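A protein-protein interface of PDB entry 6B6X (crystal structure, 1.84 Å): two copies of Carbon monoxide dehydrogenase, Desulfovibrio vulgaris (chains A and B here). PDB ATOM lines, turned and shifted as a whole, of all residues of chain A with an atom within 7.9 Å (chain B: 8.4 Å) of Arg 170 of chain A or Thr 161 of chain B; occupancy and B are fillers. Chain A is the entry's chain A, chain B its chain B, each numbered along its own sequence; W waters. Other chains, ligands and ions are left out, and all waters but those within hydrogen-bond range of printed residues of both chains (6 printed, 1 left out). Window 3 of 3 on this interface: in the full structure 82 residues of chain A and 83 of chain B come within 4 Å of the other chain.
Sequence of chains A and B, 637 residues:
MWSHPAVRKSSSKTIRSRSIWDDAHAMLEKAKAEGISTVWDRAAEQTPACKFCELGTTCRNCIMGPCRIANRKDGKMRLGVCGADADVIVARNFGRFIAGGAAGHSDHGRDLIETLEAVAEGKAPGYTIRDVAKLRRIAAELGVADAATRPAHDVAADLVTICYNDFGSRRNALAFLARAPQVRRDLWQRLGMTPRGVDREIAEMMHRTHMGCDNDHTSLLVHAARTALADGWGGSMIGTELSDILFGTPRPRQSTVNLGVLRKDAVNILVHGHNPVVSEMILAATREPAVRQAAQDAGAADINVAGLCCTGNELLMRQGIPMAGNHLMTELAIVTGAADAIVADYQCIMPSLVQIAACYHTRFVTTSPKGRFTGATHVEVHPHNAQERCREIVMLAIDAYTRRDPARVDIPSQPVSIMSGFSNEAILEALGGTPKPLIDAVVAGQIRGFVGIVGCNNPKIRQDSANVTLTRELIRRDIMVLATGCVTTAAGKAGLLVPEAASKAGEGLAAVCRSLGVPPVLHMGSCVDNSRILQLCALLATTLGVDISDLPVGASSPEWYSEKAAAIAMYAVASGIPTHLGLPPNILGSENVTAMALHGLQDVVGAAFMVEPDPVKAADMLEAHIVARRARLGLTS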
ATOM      1  N   ASN A 165      15.529  17.776 -15.530  1.00  0.00           N
ATOM      2  CA  ASN A 165      14.620  16.703 -15.932  1.00  0.00           C
ATOM      3  C   ASN A 165      15.005  15.370 -15.299  1.00  0.00           C
ATOM      4  O   ASN A 165      14.137  14.515 -15.078  1.00  0.00           O
ATOM      5  CB  ASN A 165      14.576  16.584 -17.459  1.00  0.00           C
ATOM      6  CG  ASN A 165      13.842  17.742 -18.111  1.00  0.00           C
ATOM      7  OD1 ASN A 165      13.073  18.450 -17.460  1.00  0.00           O
ATOM      8  ND2 ASN A 165      14.077  17.941 -19.404  1.00  0.00           N
ATOM      9  N   ASP A 166      16.290  15.167 -15.002  1.00  0.00           N
ATOM     10  CA  ASP A 166      16.699  13.991 -14.241  1.00  0.00           C
ATOM     11  C   ASP A 166      16.252  14.065 -12.785  1.00  0.00           C
ATOM     12  O   ASP A 166      16.186  13.028 -12.115  1.00  0.00           O
ATOM     13  CB  ASP A 166      18.215  13.799 -14.317  1.00  0.00           C
ATOM     14  CG  ASP A 166      18.639  12.963 -15.525  1.00  0.00           C
ATOM     15  OD1 ASP A 166      17.807  12.743 -16.426  1.00  0.00           O
ATOM     16  OD2 ASP A 166      19.800  12.518 -15.568  1.00  0.00           O
ATOM     17  N   PHE A 167      15.956  15.265 -12.282  1.00  0.00           N
ATOM     18  CA  PHE A 167      15.295  15.445 -10.998  1.00  0.00           C
ATOM     19  C   PHE A 167      13.779  15.515 -11.139  1.00  0.00           C
ATOM     20  O   PHE A 167      13.096  15.984 -10.220  1.00  0.00           O
ATOM     21  CB  PHE A 167      15.820  16.705 -10.298  1.00  0.00           C
ATOM     22  CG  PHE A 167      17.164  16.519  -9.655  1.00  0.00           C
ATOM     23  CD1 PHE A 167      18.325  16.556 -10.416  1.00  0.00           C
ATOM     24  CD2 PHE A 167      17.270  16.305  -8.283  1.00  0.00           C
ATOM     25  CE1 PHE A 167      19.569  16.377  -9.822  1.00  0.00           C
ATOM     26  CE2 PHE A 167      18.508  16.134  -7.681  1.00  0.00           C
ATOM     27  CZ  PHE A 167      19.660  16.168  -8.452  1.00  0.00           C
ATOM     28  N   GLY A 168      13.247  15.078 -12.282  1.00  0.00           N
ATOM     29  CA  GLY A 168      11.824  14.958 -12.485  1.00  0.00           C
ATOM     30  C   GLY A 168      11.382  13.511 -12.602  1.00  0.00           C
ATOM     31  O   GLY A 168      12.127  12.571 -12.318  1.00  0.00           O
ATOM     32  N   SER A 169      10.139  13.340 -13.047  1.00  0.00           N
ATOM     33  CA  SER A 169       9.487  12.038 -12.978  1.00  0.00           C
ATOM     34  C   SER A 169       9.086  11.497 -14.346  1.00  0.00           C
ATOM     35  O   SER A 169       8.248  10.595 -14.421  1.00  0.00           O
ATOM     36  CB  SER A 169       8.262  12.119 -12.059  1.00  0.00           C
ATOM     37  OG  SER A 169       7.793  10.822 -11.722  1.00  0.00           O
ATOM     38  N   ARG A 170       9.661  12.007 -15.434  1.00  0.00           N
ATOM     39  CA  ARG A 170       9.227  11.597 -16.767  1.00  0.00           C
ATOM     40  C   ARG A 170      10.272  10.800 -17.539  1.00  0.00           C
ATOM     41  O   ARG A 170       9.981  10.343 -18.650  1.00  0.00           O
ATOM     42  CB  ARG A 170       8.802  12.819 -17.594  1.00  0.00           C
ATOM     43  CG  ARG A 170       7.704  13.650 -16.938  1.00  0.00           C
ATOM     44  CD  ARG A 170       7.120  14.699 -17.872  1.00  0.00           C
ATOM     45  NE  ARG A 170       6.119  14.118 -18.763  1.00  0.00           N
ATOM     46  CZ  ARG A 170       5.206  14.824 -19.427  1.00  0.00           C
ATOM     47  NH1 ARG A 170       5.162  16.144 -19.304  1.00  0.00           N
ATOM     48  NH2 ARG A 170       4.329  14.203 -20.207  1.00  0.00           N
ATOM     49  N   ARG A 171      11.465  10.601 -16.995  1.00  0.00           N
ATOM     50  CA  ARG A 171      12.512   9.912 -17.737  1.00  0.00           C
ATOM     51  C   ARG A 171      12.386   8.402 -17.575  1.00  0.00           C
ATOM     52  O   ARG A 171      11.890   7.903 -16.562  1.00  0.00           O
ATOM     53  CB  ARG A 171      13.903  10.350 -17.272  1.00  0.00           C
ATOM     54  CG  ARG A 171      14.078  11.850 -17.099  1.00  0.00           C
ATOM     55  CD  ARG A 171      13.759  12.601 -18.377  1.00  0.00           C
ATOM     56  NE  ARG A 171      14.649  12.229 -19.471  1.00  0.00           N
ATOM     57  CZ  ARG A 171      14.452  12.573 -20.740  1.00  0.00           C
ATOM     58  NH1 ARG A 171      15.313  12.193 -21.674  1.00  0.00           N
ATOM     59  NH2 ARG A 171      13.392  13.296 -21.074  1.00  0.00           N
ATOM     60  N   ASN A 172      12.862   7.675 -18.584  1.00  0.00           N
ATOM     61  CA  ASN A 172      13.031   6.236 -18.454  1.00  0.00           C
ATOM     62  C   ASN A 172      14.411   5.851 -17.934  1.00  0.00           C
ATOM     63  O   ASN A 172      14.571   4.752 -17.389  1.00  0.00           O
ATOM     64  CB  ASN A 172      12.772   5.555 -19.799  1.00  0.00           C
ATOM     65  CG  ASN A 172      11.303   5.585 -20.189  1.00  0.00           C
ATOM     66  OD1 ASN A 172      10.425   5.350 -19.357  1.00  0.00           O
ATOM     67  ND2 ASN A 172      11.031   5.883 -21.450  1.00  0.00           N
ATOM     68  N   ALA A 173      15.402   6.727 -18.087  1.00  0.00           N
ATOM     69  CA  ALA A 173      16.749   6.485 -17.592  1.00  0.00           C
ATOM     70  C   ALA A 173      17.446   7.826 -17.449  1.00  0.00           C
ATOM     71  O   ALA A 173      17.209   8.745 -18.233  1.00  0.00           O
ATOM     72  CB  ALA A 173      17.550   5.571 -18.530  1.00  0.00           C
ATOM     73  N   ARG A 196      15.824   6.179 -12.849  1.00  0.00           N
ATOM     74  CA  ARG A 196      14.980   7.000 -13.713  1.00  0.00           C
ATOM     75  C   ARG A 196      14.948   8.463 -13.318  1.00  0.00           C
ATOM     76  O   ARG A 196      14.903   9.335 -14.186  1.00  0.00           O
ATOM     77  CB  ARG A 196      13.542   6.469 -13.707  1.00  0.00           C
ATOM     78  CG  ARG A 196      13.408   5.017 -14.116  1.00  0.00           C
ATOM     79  CD  ARG A 196      12.117   4.434 -13.546  1.00  0.00           C
ATOM     80  NE  ARG A 196      12.152   4.372 -12.087  1.00  0.00           N
ATOM     81  CZ  ARG A 196      11.175   3.864 -11.344  1.00  0.00           C
ATOM     82  NH1 ARG A 196      10.088   3.369 -11.929  1.00  0.00           N
ATOM     83  NH2 ARG A 196      11.285   3.841 -10.023  1.00  0.00           N
ATOM     84  N   GLY A 197      14.937   8.749 -12.026  1.00  0.00           N
ATOM     85  CA  GLY A 197      14.851  10.111 -11.548  1.00  0.00           C
ATOM     86  C   GLY A 197      15.563  10.188 -10.220  1.00  0.00           C
ATOM     87  O   GLY A 197      15.410   9.292  -9.387  1.00  0.00           O
ATOM     88  N   ARG A 200      13.085  10.774  -7.576  1.00  0.00           N
ATOM     89  CA  ARG A 200      12.026   9.770  -7.657  1.00  0.00           C
ATOM     90  C   ARG A 200      12.416   8.478  -6.944  1.00  0.00           C
ATOM     91  O   ARG A 200      11.609   7.900  -6.204  1.00  0.00           O
ATOM     92  CB  ARG A 200      11.664   9.483  -9.115  1.00  0.00           C
ATOM     93  CG  ARG A 200      10.644   8.327  -9.218  1.00  0.00           C
ATOM     94  CD  ARG A 200      10.170   8.025 -10.637  1.00  0.00           C
ATOM     95  NE  ARG A 200       9.109   7.011 -10.595  1.00  0.00           N
ATOM     96  CZ  ARG A 200       8.468   6.542 -11.659  1.00  0.00           C
ATOM     97  NH1 ARG A 200       8.776   6.984 -12.872  1.00  0.00           N
ATOM     98  NH2 ARG A 200       7.512   5.630 -11.507  1.00  0.00           N
ATOM     99  N   ARG B 110       1.555   9.962  -8.253  1.00  0.00           N
ATOM    100  CA  ARG B 110       2.363   9.782  -9.458  1.00  0.00           C
ATOM    101  C   ARG B 110       1.768   8.718 -10.375  1.00  0.00           C
ATOM    102  O   ARG B 110       1.730   8.892 -11.599  1.00  0.00           O
ATOM    103  CB  ARG B 110       3.796   9.408  -9.070  1.00  0.00           C
ATOM    104  CG  ARG B 110       4.795   9.472 -10.220  1.00  0.00           C
ATOM    105  CD  ARG B 110       6.014   8.587  -9.963  1.00  0.00           C
ATOM    106  NE  ARG B 110       6.464   8.667  -8.575  1.00  0.00           N
ATOM    107  CZ  ARG B 110       7.278   9.604  -8.100  1.00  0.00           C
ATOM    108  NH1 ARG B 110       7.621   9.587  -6.818  1.00  0.00           N
ATOM    109  NH2 ARG B 110       7.759  10.550  -8.899  1.00  0.00           N
ATOM    110  N   ILE B 113      -0.987  10.153 -12.402  1.00  0.00           N
ATOM    111  CA  ILE B 113      -0.483  10.959 -13.516  1.00  0.00           C
ATOM    112  C   ILE B 113      -0.104  10.058 -14.682  1.00  0.00           C
ATOM    113  O   ILE B 113      -0.461  10.322 -15.838  1.00  0.00           O
ATOM    114  CB  ILE B 113       0.719  11.814 -13.082  1.00  0.00           C
ATOM    115  CG1 ILE B 113       0.370  12.736 -11.914  1.00  0.00           C
ATOM    116  CG2 ILE B 113       1.218  12.631 -14.277  1.00  0.00           C
ATOM    117  CD1 ILE B 113       1.600  13.371 -11.280  1.00  0.00           C
ATOM    118  N   LEU B 116      -3.291   8.746 -16.407  1.00  0.00           N
ATOM    119  CA  LEU B 116      -3.940   9.743 -17.255  1.00  0.00           C
ATOM    120  C   LEU B 116      -3.120  10.011 -18.511  1.00  0.00           C
ATOM    121  O   LEU B 116      -3.679  10.209 -19.598  1.00  0.00           O
ATOM    122  CB  LEU B 116      -4.168  11.033 -16.470  1.00  0.00           C
ATOM    123  CG  LEU B 116      -4.820  12.183 -17.258  1.00  0.00           C
ATOM    124  CD1 LEU B 116      -6.212  11.797 -17.761  1.00  0.00           C
ATOM    125  CD2 LEU B 116      -4.884  13.448 -16.416  1.00  0.00           C
ATOM    126  N   GLU B 117      -1.793  10.023 -18.380  1.00  0.00           N
ATOM    127  CA  GLU B 117      -0.929  10.163 -19.549  1.00  0.00           C
ATOM    128  C   GLU B 117      -1.130   9.013 -20.528  1.00  0.00           C
ATOM    129  O   GLU B 117      -1.209   9.230 -21.742  1.00  0.00           O
ATOM    130  CB  GLU B 117       0.533  10.235 -19.110  1.00  0.00           C
ATOM    131  CG  GLU B 117       1.521  10.387 -20.257  1.00  0.00           C
ATOM    132  CD  GLU B 117       2.961  10.425 -19.769  1.00  0.00           C
ATOM    133  OE1 GLU B 117       3.306   9.632 -18.866  1.00  0.00           O
ATOM    134  OE2 GLU B 117       3.739  11.254 -20.282  1.00  0.00           O
ATOM    135  N   GLU B 121      -2.513   9.293 -24.326  1.00  0.00           N
ATOM    136  CA  GLU B 121      -1.760   8.755 -25.453  1.00  0.00           C
ATOM    137  C   GLU B 121      -2.508   7.668 -26.209  1.00  0.00           C
ATOM    138  O   GLU B 121      -1.995   7.188 -27.227  1.00  0.00           O
ATOM    139  CB  GLU B 121      -0.427   8.172 -24.980  1.00  0.00           C
ATOM    140  CG  GLU B 121       0.564   9.165 -24.412  1.00  0.00           C
ATOM    141  CD  GLU B 121       1.714   8.464 -23.705  1.00  0.00           C
ATOM    142  OE1 GLU B 121       1.629   7.232 -23.509  1.00  0.00           O
ATOM    143  OE2 GLU B 121       2.700   9.137 -23.346  1.00  0.00           O
ATOM    144  N   VAL B 144      -4.087  25.559 -17.907  1.00  0.00           N
ATOM    145  CA  VAL B 144      -4.029  25.013 -19.261  1.00  0.00           C
ATOM    146  C   VAL B 144      -4.790  25.939 -20.201  1.00  0.00           C
ATOM    147  O   VAL B 144      -5.976  26.217 -19.992  1.00  0.00           O
ATOM    148  CB  VAL B 144      -4.608  23.593 -19.314  1.00  0.00           C
ATOM    149  CG1 VAL B 144      -4.734  23.133 -20.773  1.00  0.00           C
ATOM    150  CG2 VAL B 144      -3.746  22.623 -18.506  1.00  0.00           C
ATOM    151  N   ASP B 154      -5.771  16.414 -25.637  1.00  0.00           N
ATOM    152  CA  ASP B 154      -4.781  17.487 -25.565  1.00  0.00           C
ATOM    153  C   ASP B 154      -4.798  18.160 -24.200  1.00  0.00           C
ATOM    154  O   ASP B 154      -3.742  18.444 -23.624  1.00  0.00           O
ATOM    155  CB  ASP B 154      -5.041  18.525 -26.655  1.00  0.00           C
ATOM    156  CG  ASP B 154      -4.689  18.024 -28.035  1.00  0.00           C
ATOM    157  OD1 ASP B 154      -4.035  16.967 -28.134  1.00  0.00           O
ATOM    158  OD2 ASP B 154      -5.073  18.693 -29.019  1.00  0.00           O
ATOM    159  N   VAL B 155      -5.993  18.449 -23.683  1.00  0.00           N
ATOM    160  CA  VAL B 155      -6.112  19.051 -22.360  1.00  0.00           C
ATOM    161  C   VAL B 155      -5.536  18.122 -21.298  1.00  0.00           C
ATOM    162  O   VAL B 155      -4.873  18.563 -20.349  1.00  0.00           O
ATOM    163  CB  VAL B 155      -7.585  19.400 -22.077  1.00  0.00           C
ATOM    164  CG1 VAL B 155      -7.754  19.893 -20.658  1.00  0.00           C
ATOM    165  CG2 VAL B 155      -8.092  20.441 -23.080  1.00  0.00           C
ATOM    166  N   ALA B 156      -5.776  16.816 -21.443  1.00  0.00           N
ATOM    167  CA  ALA B 156      -5.235  15.858 -20.485  1.00  0.00           C
ATOM    168  C   ALA B 156      -3.711  15.833 -20.533  1.00  0.00           C
ATOM    169  O   ALA B 156      -3.050  15.819 -19.485  1.00  0.00           O
ATOM    170  CB  ALA B 156      -5.817  14.468 -20.752  1.00  0.00           C
ATOM    171  N   ALA B 157      -3.134  15.864 -21.737  1.00  0.00           N
ATOM    172  CA  ALA B 157      -1.678  15.881 -21.853  1.00  0.00           C
ATOM    173  C   ALA B 157      -1.084  17.119 -21.190  1.00  0.00           C
ATOM    174  O   ALA B 157      -0.028  17.041 -20.551  1.00  0.00           O
ATOM    175  CB  ALA B 157      -1.261  15.805 -23.323  1.00  0.00           C
ATOM    176  N   ASP B 158      -1.751  18.271 -21.320  1.00  0.00           N
ATOM    177  CA  ASP B 158      -1.229  19.486 -20.696  1.00  0.00           C
ATOM    178  C   ASP B 158      -1.378  19.438 -19.180  1.00  0.00           C
ATOM    179  O   ASP B 158      -0.491  19.899 -18.453  1.00  0.00           O
ATOM    180  CB  ASP B 158      -1.924  20.720 -21.269  1.00  0.00           C
ATOM    181  CG  ASP B 158      -1.409  21.085 -22.649  1.00  0.00           C
ATOM    182  OD1 ASP B 158      -0.436  20.451 -23.107  1.00  0.00           O
ATOM    183  OD2 ASP B 158      -1.980  22.002 -23.276  1.00  0.00           O
ATOM    184  N   LEU B 159      -2.490  18.887 -18.684  1.00  0.00           N
ATOM    185  CA  LEU B 159      -2.646  18.722 -17.242  1.00  0.00           C
ATOM    186  C   LEU B 159      -1.616  17.746 -16.685  1.00  0.00           C
ATOM    187  O   LEU B 159      -1.048  17.978 -15.610  1.00  0.00           O
ATOM    188  CB  LEU B 159      -4.066  18.250 -16.913  1.00  0.00           C
ATOM    189  CG  LEU B 159      -4.339  17.914 -15.445  1.00  0.00           C
ATOM    190  CD1 LEU B 159      -4.101  19.132 -14.557  1.00  0.00           C
ATOM    191  CD2 LEU B 159      -5.772  17.391 -15.273  1.00  0.00           C
ATOM    192  N   VAL B 160      -1.367  16.645 -17.401  1.00  0.00           N
ATOM    193  CA  VAL B 160      -0.318  15.703 -17.013  1.00  0.00           C
ATOM    194  C   VAL B 160       1.016  16.425 -16.864  1.00  0.00           C
ATOM    195  O   VAL B 160       1.765  16.197 -15.907  1.00  0.00           O
ATOM    196  CB  VAL B 160      -0.232  14.556 -18.041  1.00  0.00           C
ATOM    197  CG1 VAL B 160       1.108  13.842 -17.952  1.00  0.00           C
ATOM    198  CG2 VAL B 160      -1.383  13.567 -17.831  1.00  0.00           C
ATOM    199  N   THR B 161       1.327  17.315 -17.805  1.00  0.00           N
ATOM    200  CA  THR B 161       2.593  18.041 -17.745  1.00  0.00           C
ATOM    201  C   THR B 161       2.673  18.923 -16.504  1.00  0.00           C
ATOM    202  O   THR B 161       3.722  18.993 -15.851  1.00  0.00           O
ATOM    203  CB  THR B 161       2.772  18.866 -19.019  1.00  0.00           C
ATOM    204  OG1 THR B 161       2.978  17.976 -20.121  1.00  0.00           O
ATOM    205  CG2 THR B 161       3.973  19.814 -18.903  1.00  0.00           C
ATOM    206  N   ILE B 162       1.575  19.601 -16.155  1.00  0.00           N
ATOM    207  CA  ILE B 162       1.561  20.426 -14.949  1.00  0.00           C
ATOM    208  C   ILE B 162       1.764  19.562 -13.710  1.00  0.00           C
ATOM    209  O   ILE B 162       2.521  19.920 -12.800  1.00  0.00           O
ATOM    210  CB  ILE B 162       0.251  21.231 -14.866  1.00  0.00           C
ATOM    211  CG1 ILE B 162       0.185  22.276 -15.986  1.00  0.00           C
ATOM    212  CG2 ILE B 162       0.106  21.887 -13.499  1.00  0.00           C
ATOM    213  CD1 ILE B 162      -1.135  23.010 -16.038  1.00  0.00           C
ATOM    214  N   CYS B 163       1.094  18.410 -13.656  1.00  0.00           N
ATOM    215  CA  CYS B 163       1.230  17.544 -12.490  1.00  0.00           C
ATOM    216  C   CYS B 163       2.643  16.972 -12.379  1.00  0.00           C
ATOM    217  O   CYS B 163       3.207  16.916 -11.280  1.00  0.00           O
ATOM    218  CB  CYS B 163       0.181  16.432 -12.548  1.00  0.00           C
ATOM    219  SG  CYS B 163      -1.525  17.057 -12.343  1.00  0.00           S
ATOM    220  N   TYR B 164       3.236  16.551 -13.500  1.00  0.00           N
ATOM    221  CA  TYR B 164       4.615  16.069 -13.456  1.00  0.00           C
ATOM    222  C   TYR B 164       5.585  17.169 -13.042  1.00  0.00           C
ATOM    223  O   TYR B 164       6.584  16.898 -12.364  1.00  0.00           O
ATOM    224  CB  TYR B 164       5.020  15.506 -14.812  1.00  0.00           C
ATOM    225  CG  TYR B 164       4.770  14.030 -14.994  1.00  0.00           C
ATOM    226  CD1 TYR B 164       5.093  13.113 -13.996  1.00  0.00           C
ATOM    227  CD2 TYR B 164       4.218  13.548 -16.173  1.00  0.00           C
ATOM    228  CE1 TYR B 164       4.872  11.746 -14.185  1.00  0.00           C
ATOM    229  CE2 TYR B 164       3.999  12.199 -16.366  1.00  0.00           C
ATOM    230  CZ  TYR B 164       4.326  11.307 -15.372  1.00  0.00           C
ATOM    231  OH  TYR B 164       4.096   9.967 -15.574  1.00  0.00           O
ATOM    232  N   ASN B 165       5.323  18.414 -13.440  1.00  0.00           N
ATOM    233  CA  ASN B 165       6.227  19.488 -13.046  1.00  0.00           C
ATOM    234  C   ASN B 165       6.211  19.704 -11.538  1.00  0.00           C
ATOM    235  O   ASN B 165       7.223  20.120 -10.968  1.00  0.00           O
ATOM    236  CB  ASN B 165       5.880  20.780 -13.785  1.00  0.00           C
ATOM    237  CG  ASN B 165       6.268  20.731 -15.252  1.00  0.00           C
ATOM    238  OD1 ASN B 165       7.044  19.871 -15.675  1.00  0.00           O
ATOM    239  ND2 ASN B 165       5.729  21.653 -16.035  1.00  0.00           N
ATOM    240  N   ASP B 166       5.085  19.418 -10.874  1.00  0.00           N
ATOM    241  CA  ASP B 166       5.071  19.425  -9.416  1.00  0.00           C
ATOM    242  C   ASP B 166       5.886  18.278  -8.826  1.00  0.00           C
ATOM    243  O   ASP B 166       6.244  18.335  -7.645  1.00  0.00           O
ATOM    244  CB  ASP B 166       3.632  19.366  -8.892  1.00  0.00           C
ATOM    245  CG  ASP B 166       2.985  20.743  -8.806  1.00  0.00           C
ATOM    246  OD1 ASP B 166       3.555  21.713  -9.352  1.00  0.00           O
ATOM    247  OD2 ASP B 166       1.912  20.858  -8.185  1.00  0.00           O
ATOM    248  N   PHE B 167       6.177  17.239  -9.613  1.00  0.00           N
ATOM    249  CA  PHE B 167       7.108  16.184  -9.228  1.00  0.00           C
ATOM    250  C   PHE B 167       8.509  16.443  -9.770  1.00  0.00           C
ATOM    251  O   PHE B 167       9.325  15.518  -9.842  1.00  0.00           O
ATOM    252  CB  PHE B 167       6.608  14.819  -9.705  1.00  0.00           C
ATOM    253  CG  PHE B 167       5.517  14.234  -8.851  1.00  0.00           C
ATOM    254  CD1 PHE B 167       4.205  14.668  -8.981  1.00  0.00           C
ATOM    255  CD2 PHE B 167       5.801  13.234  -7.928  1.00  0.00           C
ATOM    256  CE1 PHE B 167       3.201  14.130  -8.194  1.00  0.00           C
ATOM    257  CE2 PHE B 167       4.795  12.684  -7.138  1.00  0.00           C
ATOM    258  CZ  PHE B 167       3.494  13.135  -7.274  1.00  0.00           C
ATOM    259  N   GLY B 168       8.784  17.679 -10.185  1.00  0.00           N
ATOM    260  CA  GLY B 168      10.111  18.103 -10.553  1.00  0.00           C
ATOM    261  C   GLY B 168      10.692  19.070  -9.540  1.00  0.00           C
ATOM    262  O   GLY B 168      10.171  19.259  -8.438  1.00  0.00           O
ATOM    263  N   ARG B 171       9.776  24.299  -9.548  1.00  0.00           N
ATOM    264  CA  ARG B 171       8.679  25.152  -9.108  1.00  0.00           C
ATOM    265  C   ARG B 171       9.054  25.899  -7.835  1.00  0.00           C
ATOM    266  O   ARG B 171       9.845  25.420  -7.019  1.00  0.00           O
ATOM    267  CB  ARG B 171       7.403  24.343  -8.848  1.00  0.00           C
ATOM    268  CG  ARG B 171       7.081  23.276  -9.881  1.00  0.00           C
ATOM    269  CD  ARG B 171       6.897  23.877 -11.257  1.00  0.00           C
ATOM    270  NE  ARG B 171       5.855  24.899 -11.270  1.00  0.00           N
ATOM    271  CZ  ARG B 171       5.587  25.674 -12.313  1.00  0.00           C
ATOM    272  NH1 ARG B 171       4.623  26.582 -12.239  1.00  0.00           N
ATOM    273  NH2 ARG B 171       6.287  25.541 -13.434  1.00  0.00           N
ATOM    274  N   ALA B 175       1.217  23.469  -7.686  1.00  0.00           N
ATOM    275  CA  ALA B 175       0.132  24.041  -8.483  1.00  0.00           C
ATOM    276  C   ALA B 175      -1.156  24.205  -7.679  1.00  0.00           C
ATOM    277  O   ALA B 175      -1.824  25.240  -7.775  1.00  0.00           O
ATOM    278  CB  ALA B 175      -0.119  23.173  -9.715  1.00  0.00           C
ATOM    279  N   ASP B 199       8.344  15.194  -4.793  1.00  0.00           N
ATOM    280  CA  ASP B 199       9.505  14.368  -4.475  1.00  0.00           C
ATOM    281  C   ASP B 199      10.613  15.184  -3.821  1.00  0.00           C
ATOM    282  O   ASP B 199      11.348  14.661  -2.974  1.00  0.00           O
ATOM    283  CB  ASP B 199      10.051  13.689  -5.733  1.00  0.00           C
ATOM    284  CG  ASP B 199       9.166  12.560  -6.228  1.00  0.00           C
ATOM    285  OD1 ASP B 199       8.312  12.079  -5.448  1.00  0.00           O
ATOM    286  OD2 ASP B 199       9.350  12.139  -7.396  1.00  0.00           O
ATOM    287  N   LEU B 242      -7.175  13.642 -10.095  1.00  0.00           N
ATOM    288  CA  LEU B 242      -6.995  12.804 -11.276  1.00  0.00           C
ATOM    289  C   LEU B 242      -7.805  11.518 -11.184  1.00  0.00           C
ATOM    290  O   LEU B 242      -8.294  11.024 -12.207  1.00  0.00           O
ATOM    291  CB  LEU B 242      -5.513  12.486 -11.486  1.00  0.00           C
ATOM    292  CG  LEU B 242      -4.639  13.692 -11.837  1.00  0.00           C
ATOM    293  CD1 LEU B 242      -3.254  13.248 -12.275  1.00  0.00           C
ATOM    294  CD2 LEU B 242      -5.309  14.526 -12.920  1.00  0.00           C
HETATM  295  O   HOH W   1       6.015   8.377 -13.690  1.00  0.00           O
HETATM  296  O   HOH W   2       8.666  15.618 -13.708  1.00  0.00           O
HETATM  297  O   HOH W   3       7.888   5.671  -8.388  1.00  0.00           O
HETATM  298  O   HOH W   4       6.109  11.233 -19.434  1.00  0.00           O
HETATM  299  O   HOH W   5       2.005  15.255 -21.540  1.00  0.00           O
HETATM  300  O   HOH W   6      12.165  16.579  -7.635  1.00  0.00           O
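The side-chain hydroxyl of Ser 169 of chain A lies within hydrogen-bond range of the guanidinium group of Arg 110 of chain B, at 2.8 Å.
The guanidinium group (NH1) of Arg 170 of chain A sits at hydrogen-bond distance from the side-chain hydroxyl (OG1) of Thr 161 of chain B (3.0 Å).
The guanidinium group (NH2) of Arg 170 of chain A is in salt-bridge range of the side-chain carboxylate (OE2) of Glu 117 of chain B (3.0 Å).
OE1 of Glu 117 of chain B lies within hydrogen-bond range of OH of Tyr 164 of chain B.
ND2 of Asn 165 of chain B sits close to O of Thr 161 of chain B, 3.3 Å away.
The side-chain carboxylate of Asp 199 of chain B lies within salt-bridge range of the guanidinium group of Arg 110 of chain B (2.7 Å).
Among the printed residues, pairs that only touch across the chains: Phe 167 of chain A with Phe 167 of chain B (3.8 Å), Phe 167 of chain A with Gly 168 of chain B (3.7 Å), Gly 168 of chain A with Phe 167 of chain B (3.7 Å), Ser 169 of chain A with Tyr 164 of chain B (3.6 Å), Ser 169 of chain A with Phe 167 of chain B (3.9 Å), Arg 170 of chain A with Val 160 of chain B (3.9 Å), Arg 170 of chain A with Tyr 164 of chain B (3.3 Å), Arg 200 of chain A with Arg 110 of chain B (3.5 Å) and Arg 200 of chain A with Asp 199 of chain B (3.6 Å).
Printed residues of chain B within 4 Å of Arg 170 of chain A: Glu 117 (3.0 Å), Val 160 (3.9 Å), Thr 161 (3.0 Å) and Tyr 164 (3.3 Å).
Ser 169 of chain A touches three residues of chain B.
Of the printed residues of chain A, Val 160 of chain B touches Arg 170.
Of the printed residues of chain B, Phe 167 of chain A touches Phe 167 and Gly 168.
Asn 165 of chain A touches none of the printed residues of chain B.
Along chain A the printed residues that touch a printed residue of chain B span positions 167 to 200.
Among the printed residues, 12 pairs touch across the chains.
Among the printed residues, Asp or Glu carboxylates within 4 Å of a Lys or Arg side-chain nitrogen of the other chain: Arg 170 of chain A with Glu 117 of chain B (3.0 Å).
Phe 167 of chain B touches its own counterpart, Phe 167 of chain A.
Phe 167 of chain A touches Gly 168 of chain B, and with the chains exchanged Gly 168 of chain A touches Phe 167 of chain B.
Water W5 lies within hydrogen-bond range of the guanidinium group (NH2) of Arg 170 of chain A (2.9 Å), the backbone carbonyl oxygen (O) of Ala 157 of chain B (2.9 Å) and the side-chain hydroxyl (OG1) of Thr 161 of chain B (3.2 Å).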
